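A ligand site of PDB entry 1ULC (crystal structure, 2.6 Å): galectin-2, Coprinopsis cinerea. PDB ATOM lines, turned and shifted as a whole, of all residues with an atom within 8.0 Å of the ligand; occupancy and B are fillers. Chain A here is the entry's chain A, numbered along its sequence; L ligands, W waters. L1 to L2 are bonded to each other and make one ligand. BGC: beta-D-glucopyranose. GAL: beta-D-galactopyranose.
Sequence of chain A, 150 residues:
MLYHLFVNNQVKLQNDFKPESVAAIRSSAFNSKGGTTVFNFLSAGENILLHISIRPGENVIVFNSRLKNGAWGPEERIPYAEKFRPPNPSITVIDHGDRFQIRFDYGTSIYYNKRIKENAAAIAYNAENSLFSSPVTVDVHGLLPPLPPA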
ATOM      1  N   THR A  36      36.267 -20.579  15.117  1.00  0.00           N
ATOM      2  CA  THR A  36      35.594 -20.298  13.859  1.00  0.00           C
ATOM      3  C   THR A  36      36.480 -19.523  12.899  1.00  0.00           C
ATOM      4  O   THR A  36      37.041 -18.475  13.250  1.00  0.00           O
ATOM      5  CB  THR A  36      34.283 -19.547  14.102  1.00  0.00           C
ATOM      6  OG1 THR A  36      33.361 -20.442  14.740  1.00  0.00           O
ATOM      7  CG2 THR A  36      33.679 -19.057  12.798  1.00  0.00           C
ATOM      8  N   VAL A  38      36.605 -17.953   8.935  1.00  0.00           N
ATOM      9  CA  VAL A  38      35.775 -17.526   7.820  1.00  0.00           C
ATOM     10  C   VAL A  38      36.534 -17.114   6.566  1.00  0.00           C
ATOM     11  O   VAL A  38      37.625 -16.541   6.652  1.00  0.00           O
ATOM     12  CB  VAL A  38      34.865 -16.339   8.251  1.00  0.00           C
ATOM     13  CG1 VAL A  38      34.170 -15.741   7.047  1.00  0.00           C
ATOM     14  CG2 VAL A  38      33.846 -16.820   9.263  1.00  0.00           C
ATOM     15  N   ASN A  40      35.462 -15.268   2.844  1.00  0.00           N
ATOM     16  CA  ASN A  40      34.425 -14.636   2.023  1.00  0.00           C
ATOM     17  C   ASN A  40      34.897 -14.297   0.624  1.00  0.00           C
ATOM     18  O   ASN A  40      36.024 -13.841   0.436  1.00  0.00           O
ATOM     19  CB  ASN A  40      33.952 -13.313   2.648  1.00  0.00           C
ATOM     20  CG  ASN A  40      33.229 -13.506   3.952  1.00  0.00           C
ATOM     21  OD1 ASN A  40      32.364 -14.362   4.085  1.00  0.00           O
ATOM     22  ND2 ASN A  40      33.579 -12.683   4.931  1.00  0.00           N
ATOM     23  N   HIS A  51      29.944 -17.047   1.435  1.00  0.00           N
ATOM     24  CA  HIS A  51      30.425 -16.986   2.816  1.00  0.00           C
ATOM     25  C   HIS A  51      30.616 -18.414   3.311  1.00  0.00           C
ATOM     26  O   HIS A  51      29.691 -19.237   3.231  1.00  0.00           O
ATOM     27  CB  HIS A  51      29.399 -16.268   3.710  1.00  0.00           C
ATOM     28  CG  HIS A  51      29.713 -16.306   5.188  1.00  0.00           C
ATOM     29  ND1 HIS A  51      30.748 -15.587   5.744  1.00  0.00           N
ATOM     30  CD2 HIS A  51      29.111 -16.959   6.205  1.00  0.00           C
ATOM     31  CE1 HIS A  51      30.766 -15.798   7.054  1.00  0.00           C
ATOM     32  NE2 HIS A  51      29.793 -16.623   7.357  1.00  0.00           N
ATOM     33  N   ILE A  52      31.811 -18.709   3.800  1.00  0.00           N
ATOM     34  CA  ILE A  52      32.122 -20.024   4.329  1.00  0.00           C
ATOM     35  C   ILE A  52      32.515 -19.835   5.790  1.00  0.00           C
ATOM     36  O   ILE A  52      33.501 -19.179   6.108  1.00  0.00           O
ATOM     37  CB  ILE A  52      33.305 -20.697   3.602  1.00  0.00           C
ATOM     38  CG1 ILE A  52      33.095 -20.635   2.087  1.00  0.00           C
ATOM     39  CG2 ILE A  52      33.414 -22.146   4.019  1.00  0.00           C
ATOM     40  CD1 ILE A  52      34.250 -21.241   1.275  1.00  0.00           C
ATOM     41  N   SER A  53      31.713 -20.406   6.680  1.00  0.00           N
ATOM     42  CA  SER A  53      31.963 -20.294   8.102  1.00  0.00           C
ATOM     43  C   SER A  53      32.304 -21.689   8.623  1.00  0.00           C
ATOM     44  O   SER A  53      31.433 -22.554   8.736  1.00  0.00           O
ATOM     45  CB  SER A  53      30.738 -19.733   8.823  1.00  0.00           C
ATOM     46  OG  SER A  53      30.998 -19.511  10.196  1.00  0.00           O
ATOM     47  N   ILE A  54      33.582 -21.895   8.918  1.00  0.00           N
ATOM     48  CA  ILE A  54      34.082 -23.166   9.437  1.00  0.00           C
ATOM     49  C   ILE A  54      34.027 -23.128  10.969  1.00  0.00           C
ATOM     50  O   ILE A  54      34.858 -22.488  11.618  1.00  0.00           O
ATOM     51  CB  ILE A  54      35.521 -23.397   8.963  1.00  0.00           C
ATOM     52  CG1 ILE A  54      35.585 -23.220   7.455  1.00  0.00           C
ATOM     53  CG2 ILE A  54      35.988 -24.785   9.351  1.00  0.00           C
ATOM     54  CD1 ILE A  54      36.987 -23.121   6.927  1.00  0.00           C
ATOM     55  N   ARG A  55      33.043 -23.811  11.532  1.00  0.00           N
ATOM     56  CA  ARG A  55      32.852 -23.832  12.974  1.00  0.00           C
ATOM     57  C   ARG A  55      33.225 -25.171  13.593  1.00  0.00           C
ATOM     58  O   ARG A  55      32.431 -26.110  13.599  1.00  0.00           O
ATOM     59  CB  ARG A  55      31.403 -23.497  13.300  1.00  0.00           C
ATOM     60  CG  ARG A  55      30.921 -22.265  12.585  1.00  0.00           C
ATOM     61  CD  ARG A  55      29.424 -22.109  12.671  1.00  0.00           C
ATOM     62  NE  ARG A  55      28.992 -20.900  11.977  1.00  0.00           N
ATOM     63  CZ  ARG A  55      27.747 -20.439  11.958  1.00  0.00           C
ATOM     64  NH1 ARG A  55      26.787 -21.086  12.609  1.00  0.00           N
ATOM     65  NH2 ARG A  55      27.472 -19.333  11.295  1.00  0.00           N
ATOM     66  N   GLU A  58      31.201 -26.346  16.845  1.00  0.00           N
ATOM     67  CA  GLU A  58      29.759 -26.498  16.638  1.00  0.00           C
ATOM     68  C   GLU A  58      29.646 -27.642  15.641  1.00  0.00           C
ATOM     69  O   GLU A  58      28.556 -28.044  15.245  1.00  0.00           O
ATOM     70  CB  GLU A  58      29.237 -25.181  16.044  1.00  0.00           C
ATOM     71  CG  GLU A  58      27.774 -24.834  16.271  1.00  0.00           C
ATOM     72  CD  GLU A  58      27.430 -23.429  15.721  1.00  0.00           C
ATOM     73  OE1 GLU A  58      28.131 -22.449  16.076  1.00  0.00           O
ATOM     74  OE2 GLU A  58      26.444 -23.306  14.947  1.00  0.00           O
ATOM     75  N   VAL A  60      30.296 -27.864  12.409  1.00  0.00           N
ATOM     76  CA  VAL A  60      29.553 -27.564  11.204  1.00  0.00           C
ATOM     77  C   VAL A  60      30.243 -26.476  10.388  1.00  0.00           C
ATOM     78  O   VAL A  60      30.962 -25.632  10.929  1.00  0.00           O
ATOM     79  CB  VAL A  60      28.103 -27.126  11.544  1.00  0.00           C
ATOM     80  CG1 VAL A  60      28.117 -25.764  12.250  1.00  0.00           C
ATOM     81  CG2 VAL A  60      27.273 -27.073  10.275  1.00  0.00           C
ATOM     82  N   VAL A  62      29.204 -23.567   7.684  1.00  0.00           N
ATOM     83  CA  VAL A  62      28.017 -22.881   7.185  1.00  0.00           C
ATOM     84  C   VAL A  62      28.279 -22.049   5.936  1.00  0.00           C
ATOM     85  O   VAL A  62      29.251 -21.313   5.874  1.00  0.00           O
ATOM     86  CB  VAL A  62      27.415 -21.951   8.257  1.00  0.00           C
ATOM     87  CG1 VAL A  62      26.081 -21.401   7.788  1.00  0.00           C
ATOM     88  CG2 VAL A  62      27.260 -22.696   9.571  1.00  0.00           C
ATOM     89  N   PHE A  63      27.391 -22.173   4.957  1.00  0.00           N
ATOM     90  CA  PHE A  63      27.514 -21.429   3.709  1.00  0.00           C
ATOM     91  C   PHE A  63      26.348 -20.452   3.600  1.00  0.00           C
ATOM     92  O   PHE A  63      25.208 -20.810   3.864  1.00  0.00           O
ATOM     93  CB  PHE A  63      27.501 -22.365   2.488  1.00  0.00           C
ATOM     94  CG  PHE A  63      28.660 -23.311   2.447  1.00  0.00           C
ATOM     95  CD1 PHE A  63      28.653 -24.476   3.206  1.00  0.00           C
ATOM     96  CD2 PHE A  63      29.784 -23.029   1.676  1.00  0.00           C
ATOM     97  CE1 PHE A  63      29.742 -25.352   3.199  1.00  0.00           C
ATOM     98  CE2 PHE A  63      30.883 -23.897   1.658  1.00  0.00           C
ATOM     99  CZ  PHE A  63      30.858 -25.057   2.420  1.00  0.00           C
ATOM    100  N   ASN A  64      26.651 -19.214   3.219  1.00  0.00           N
ATOM    101  CA  ASN A  64      25.619 -18.190   3.088  1.00  0.00           C
ATOM    102  C   ASN A  64      26.104 -17.039   2.207  1.00  0.00           C
ATOM    103  O   ASN A  64      27.243 -17.025   1.741  1.00  0.00           O
ATOM    104  CB  ASN A  64      25.229 -17.653   4.469  1.00  0.00           C
ATOM    105  CG  ASN A  64      23.745 -17.292   4.558  1.00  0.00           C
ATOM    106  OD1 ASN A  64      23.116 -16.978   3.557  1.00  0.00           O
ATOM    107  ND2 ASN A  64      23.196 -17.325   5.776  1.00  0.00           N
ATOM    108  N   SER A  65      25.208 -16.073   1.981  1.00  0.00           N
ATOM    109  CA  SER A  65      25.481 -14.896   1.167  1.00  0.00           C
ATOM    110  C   SER A  65      24.713 -13.723   1.767  1.00  0.00           C
ATOM    111  O   SER A  65      23.776 -13.931   2.538  1.00  0.00           O
ATOM    112  CB  SER A  65      25.002 -15.104  -0.280  1.00  0.00           C
ATOM    113  OG  SER A  65      25.653 -16.174  -0.928  1.00  0.00           O
ATOM    114  N   ARG A  66      25.097 -12.507   1.402  1.00  0.00           N
ATOM    115  CA  ARG A  66      24.392 -11.311   1.850  1.00  0.00           C
ATOM    116  C   ARG A  66      25.019 -10.090   1.190  1.00  0.00           C
ATOM    117  O   ARG A  66      26.205 -10.086   0.887  1.00  0.00           O
ATOM    118  CB  ARG A  66      24.407 -11.167   3.383  1.00  0.00           C
ATOM    119  CG  ARG A  66      25.644 -10.531   3.963  1.00  0.00           C
ATOM    120  CD  ARG A  66      25.522 -10.382   5.479  1.00  0.00           C
ATOM    121  NE  ARG A  66      26.660  -9.669   6.038  1.00  0.00           N
ATOM    122  CZ  ARG A  66      26.818  -8.356   6.028  1.00  0.00           C
ATOM    123  NH1 ARG A  66      25.891  -7.573   5.487  1.00  0.00           N
ATOM    124  NH2 ARG A  66      27.896  -7.804   6.541  1.00  0.00           N
ATOM    125  N   ALA A  71      20.734  -8.511   5.035  1.00  0.00           N
ATOM    126  CA  ALA A  71      20.687  -9.579   6.017  1.00  0.00           C
ATOM    127  C   ALA A  71      21.153 -10.880   5.383  1.00  0.00           C
ATOM    128  O   ALA A  71      21.230 -11.002   4.160  1.00  0.00           O
ATOM    129  CB  ALA A  71      19.279  -9.739   6.545  1.00  0.00           C
ATOM    130  N   TRP A  72      21.490 -11.844   6.242  1.00  0.00           N
ATOM    131  CA  TRP A  72      21.932 -13.157   5.785  1.00  0.00           C
ATOM    132  C   TRP A  72      20.721 -13.861   5.219  1.00  0.00           C
ATOM    133  O   TRP A  72      19.587 -13.537   5.562  1.00  0.00           O
ATOM    134  CB  TRP A  72      22.475 -13.984   6.948  1.00  0.00           C
ATOM    135  CG  TRP A  72      23.787 -13.514   7.490  1.00  0.00           C
ATOM    136  CD1 TRP A  72      24.023 -12.967   8.713  1.00  0.00           C
ATOM    137  CD2 TRP A  72      25.056 -13.589   6.826  1.00  0.00           C
ATOM    138  NE1 TRP A  72      25.361 -12.695   8.870  1.00  0.00           N
ATOM    139  CE2 TRP A  72      26.014 -13.071   7.724  1.00  0.00           C
ATOM    140  CE3 TRP A  72      25.469 -14.048   5.576  1.00  0.00           C
ATOM    141  CZ2 TRP A  72      27.382 -13.001   7.403  1.00  0.00           C
ATOM    142  CZ3 TRP A  72      26.825 -13.985   5.257  1.00  0.00           C
ATOM    143  CH2 TRP A  72      27.756 -13.460   6.170  1.00  0.00           C
ATOM    144  N   GLY A  73      20.960 -14.827   4.339  1.00  0.00           N
ATOM    145  CA  GLY A  73      19.869 -15.594   3.772  1.00  0.00           C
ATOM    146  C   GLY A  73      19.789 -16.905   4.519  1.00  0.00           C
ATOM    147  O   GLY A  73      20.247 -17.008   5.656  1.00  0.00           O
ATOM    148  N   PRO A  74      19.189 -17.936   3.921  1.00  0.00           N
ATOM    149  CA  PRO A  74      19.135 -19.192   4.666  1.00  0.00           C
ATOM    150  C   PRO A  74      20.503 -19.893   4.667  1.00  0.00           C
ATOM    151  O   PRO A  74      21.249 -19.825   3.680  1.00  0.00           O
ATOM    152  CB  PRO A  74      18.040 -19.981   3.935  1.00  0.00           C
ATOM    153  CG  PRO A  74      18.103 -19.441   2.530  1.00  0.00           C
ATOM    154  CD  PRO A  74      18.322 -17.965   2.738  1.00  0.00           C
ATOM    155  N   GLU A  75      20.851 -20.546   5.777  1.00  0.00           N
ATOM    156  CA  GLU A  75      22.137 -21.223   5.874  1.00  0.00           C
ATOM    157  C   GLU A  75      22.124 -22.615   5.279  1.00  0.00           C
ATOM    158  O   GLU A  75      21.167 -23.364   5.440  1.00  0.00           O
ATOM    159  CB  GLU A  75      22.574 -21.346   7.339  1.00  0.00           C
ATOM    160  CG  GLU A  75      22.734 -20.042   8.070  1.00  0.00           C
ATOM    161  CD  GLU A  75      23.361 -20.216   9.440  1.00  0.00           C
ATOM    162  OE1 GLU A  75      23.204 -21.314  10.024  1.00  0.00           O
ATOM    163  OE2 GLU A  75      23.988 -19.256   9.940  1.00  0.00           O
ATOM    164  N   GLU A  76      23.207 -22.931   4.579  1.00  0.00           N
ATOM    165  CA  GLU A  76      23.393 -24.251   3.992  1.00  0.00           C
ATOM    166  C   GLU A  76      24.566 -24.804   4.802  1.00  0.00           C
ATOM    167  O   GLU A  76      25.671 -24.258   4.773  1.00  0.00           O
ATOM    168  CB  GLU A  76      23.706 -24.129   2.492  1.00  0.00           C
ATOM    169  CG  GLU A  76      22.484 -23.759   1.674  1.00  0.00           C
ATOM    170  CD  GLU A  76      22.744 -23.675   0.172  1.00  0.00           C
ATOM    171  OE1 GLU A  76      23.405 -24.571  -0.382  1.00  0.00           O
ATOM    172  OE2 GLU A  76      22.270 -22.713  -0.451  1.00  0.00           O
ATOM    173  N   ARG A  77      24.309 -25.873   5.546  1.00  0.00           N
ATOM    174  CA  ARG A  77      25.316 -26.465   6.434  1.00  0.00           C
ATOM    175  C   ARG A  77      25.802 -27.870   6.068  1.00  0.00           C
ATOM    176  O   ARG A  77      25.234 -28.530   5.212  1.00  0.00           O
ATOM    177  CB  ARG A  77      24.746 -26.520   7.858  1.00  0.00           C
ATOM    178  CG  ARG A  77      24.388 -25.186   8.464  1.00  0.00           C
ATOM    179  CD  ARG A  77      23.305 -25.349   9.526  1.00  0.00           C
ATOM    180  NE  ARG A  77      23.233 -24.200  10.423  1.00  0.00           N
ATOM    181  CZ  ARG A  77      23.925 -24.084  11.547  1.00  0.00           C
ATOM    182  NH1 ARG A  77      24.742 -25.058  11.929  1.00  0.00           N
ATOM    183  NH2 ARG A  77      23.811 -22.998  12.298  1.00  0.00           N
ATOM    184  N   ARG A 115      23.600 -16.742  -5.508  1.00  0.00           N
ATOM    185  CA  ARG A 115      22.436 -15.974  -5.055  1.00  0.00           C
ATOM    186  C   ARG A 115      22.537 -14.518  -5.477  1.00  0.00           C
ATOM    187  O   ARG A 115      21.513 -13.848  -5.629  1.00  0.00           O
ATOM    188  CB  ARG A 115      22.318 -16.053  -3.526  1.00  0.00           C
ATOM    189  CG  ARG A 115      22.144 -17.467  -2.979  1.00  0.00           C
ATOM    190  CD  ARG A 115      21.955 -17.435  -1.485  1.00  0.00           C
ATOM    191  NE  ARG A 115      21.862 -18.766  -0.908  1.00  0.00           N
ATOM    192  CZ  ARG A 115      21.644 -19.020   0.379  1.00  0.00           C
ATOM    193  NH1 ARG A 115      21.504 -18.028   1.243  1.00  0.00           N
ATOM    194  NH2 ARG A 115      21.585 -20.280   0.810  1.00  0.00           N
HETATM  195  C2  BGC L   1      22.358 -19.142  13.608  1.00  0.00           C
HETATM  196  C3  BGC L   1      23.845 -18.875  13.364  1.00  0.00           C
HETATM  197  C4  BGC L   1      24.032 -17.411  12.938  1.00  0.00           C
HETATM  198  C5  BGC L   1      23.395 -16.462  13.966  1.00  0.00           C
HETATM  199  C6  BGC L   1      23.376 -15.027  13.482  1.00  0.00           C
HETATM  200  C1  BGC L   1      21.880 -18.172  14.670  1.00  0.00           C
HETATM  201  O1  BGC L   1      20.534 -18.394  14.933  1.00  0.00           O
HETATM  202  O2  BGC L   1      22.160 -20.479  14.019  1.00  0.00           O
HETATM  203  O3  BGC L   1      24.339 -19.744  12.362  1.00  0.00           O
HETATM  204  O4  BGC L   1      25.441 -17.131  12.829  1.00  0.00           O
HETATM  205  O5  BGC L   1      22.016 -16.830  14.199  1.00  0.00           O
HETATM  206  O6  BGC L   1      22.682 -14.916  12.243  1.00  0.00           O
HETATM  207  C1  GAL L   2      25.834 -16.278  11.812  1.00  0.00           C
HETATM  208  C2  GAL L   2      27.295 -15.883  12.063  1.00  0.00           C
HETATM  209  C3  GAL L   2      27.867 -15.111  10.872  1.00  0.00           C
HETATM  210  C4  GAL L   2      27.630 -15.886   9.571  1.00  0.00           C
HETATM  211  C5  GAL L   2      26.152 -16.224   9.437  1.00  0.00           C
HETATM  212  C6  GAL L   2      25.881 -17.061   8.211  1.00  0.00           C
HETATM  213  O2  GAL L   2      27.369 -15.087  13.240  1.00  0.00           O
HETATM  214  O3  GAL L   2      29.259 -14.894  11.059  1.00  0.00           O
HETATM  215  O4  GAL L   2      28.394 -17.079   9.570  1.00  0.00           O
HETATM  216  O5  GAL L   2      25.710 -16.989  10.575  1.00  0.00           O
HETATM  217  O6  GAL L   2      24.503 -17.332   8.071  1.00  0.00           O
HETATM  218  O   HOH W   1      20.174 -17.810  17.770  1.00  0.00           O
HETATM  219  O   HOH W   2      30.659 -17.176  11.659  1.00  0.00           O
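The guanidinium group (NH1) of Arg 55 lies within hydrogen-bond range of an oxygen (O3) of BGC L1, at 2.8 Å.
An oxygen (O3) of BGC L1 lies within hydrogen-bond range of the guanidinium group (NH2) of Arg 77, at 3.3 Å.
A ring nitrogen (NE2) of His 51 sits at hydrogen-bond distance from an oxygen (O4) of GAL L2 (2.7 Å).
The side-chain carboxylate (OE2) of Glu 75 is in hydrogen-bond range of an oxygen (O3) of BGC L1.
The side-chain amide nitrogen of Asn 64 sits at hydrogen-bond distance from an oxygen (O6) of GAL L2, at 2.6 Å.
N of His 51 lies within hydrogen-bond range of O of Asn 64 (2.7 Å).
The backbone carbonyl oxygen (O) of Pro 74 sits close to the side-chain amide oxygen (OD1) of Asn 64.
The guanidinium group (NH2) of Arg 77 is in salt-bridge range of the side-chain carboxylate (OE2) of Glu 58 (3.7 Å).
The guanidinium group (NE) of Arg 55 is in hydrogen-bond range of the side-chain hydroxyl (OG) of Ser 53 (3.0 Å).
The side-chain amide oxygen of Asn 64 is in hydrogen-bond range of the guanidinium group of Arg 115, 3.0 Å away.
The backbone carbonyl oxygen of Gly 73 lies within hydrogen-bond range of the side-chain amide nitrogen of Asn 64 (3.0 Å).
OE1 of Glu 75 lies within salt-bridge range of NH2 of Arg 77.
The side-chain carboxylate (OE2) of Glu 75 is in salt-bridge range of the guanidinium group (NH2) of Arg 55, at 3.7 Å.
Residues that only touch the ligand: Ser 53 (3.6 Å) and Trp 72 (3.6 Å).
The nearest printed residue that does not touch the ligand is Val 62 (4.4 Å).
Water W2 bridges an oxygen (O3) of GAL L2 (2.7 Å) and the side-chain hydroxyl (OG) of Ser 53 (2.8 Å).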
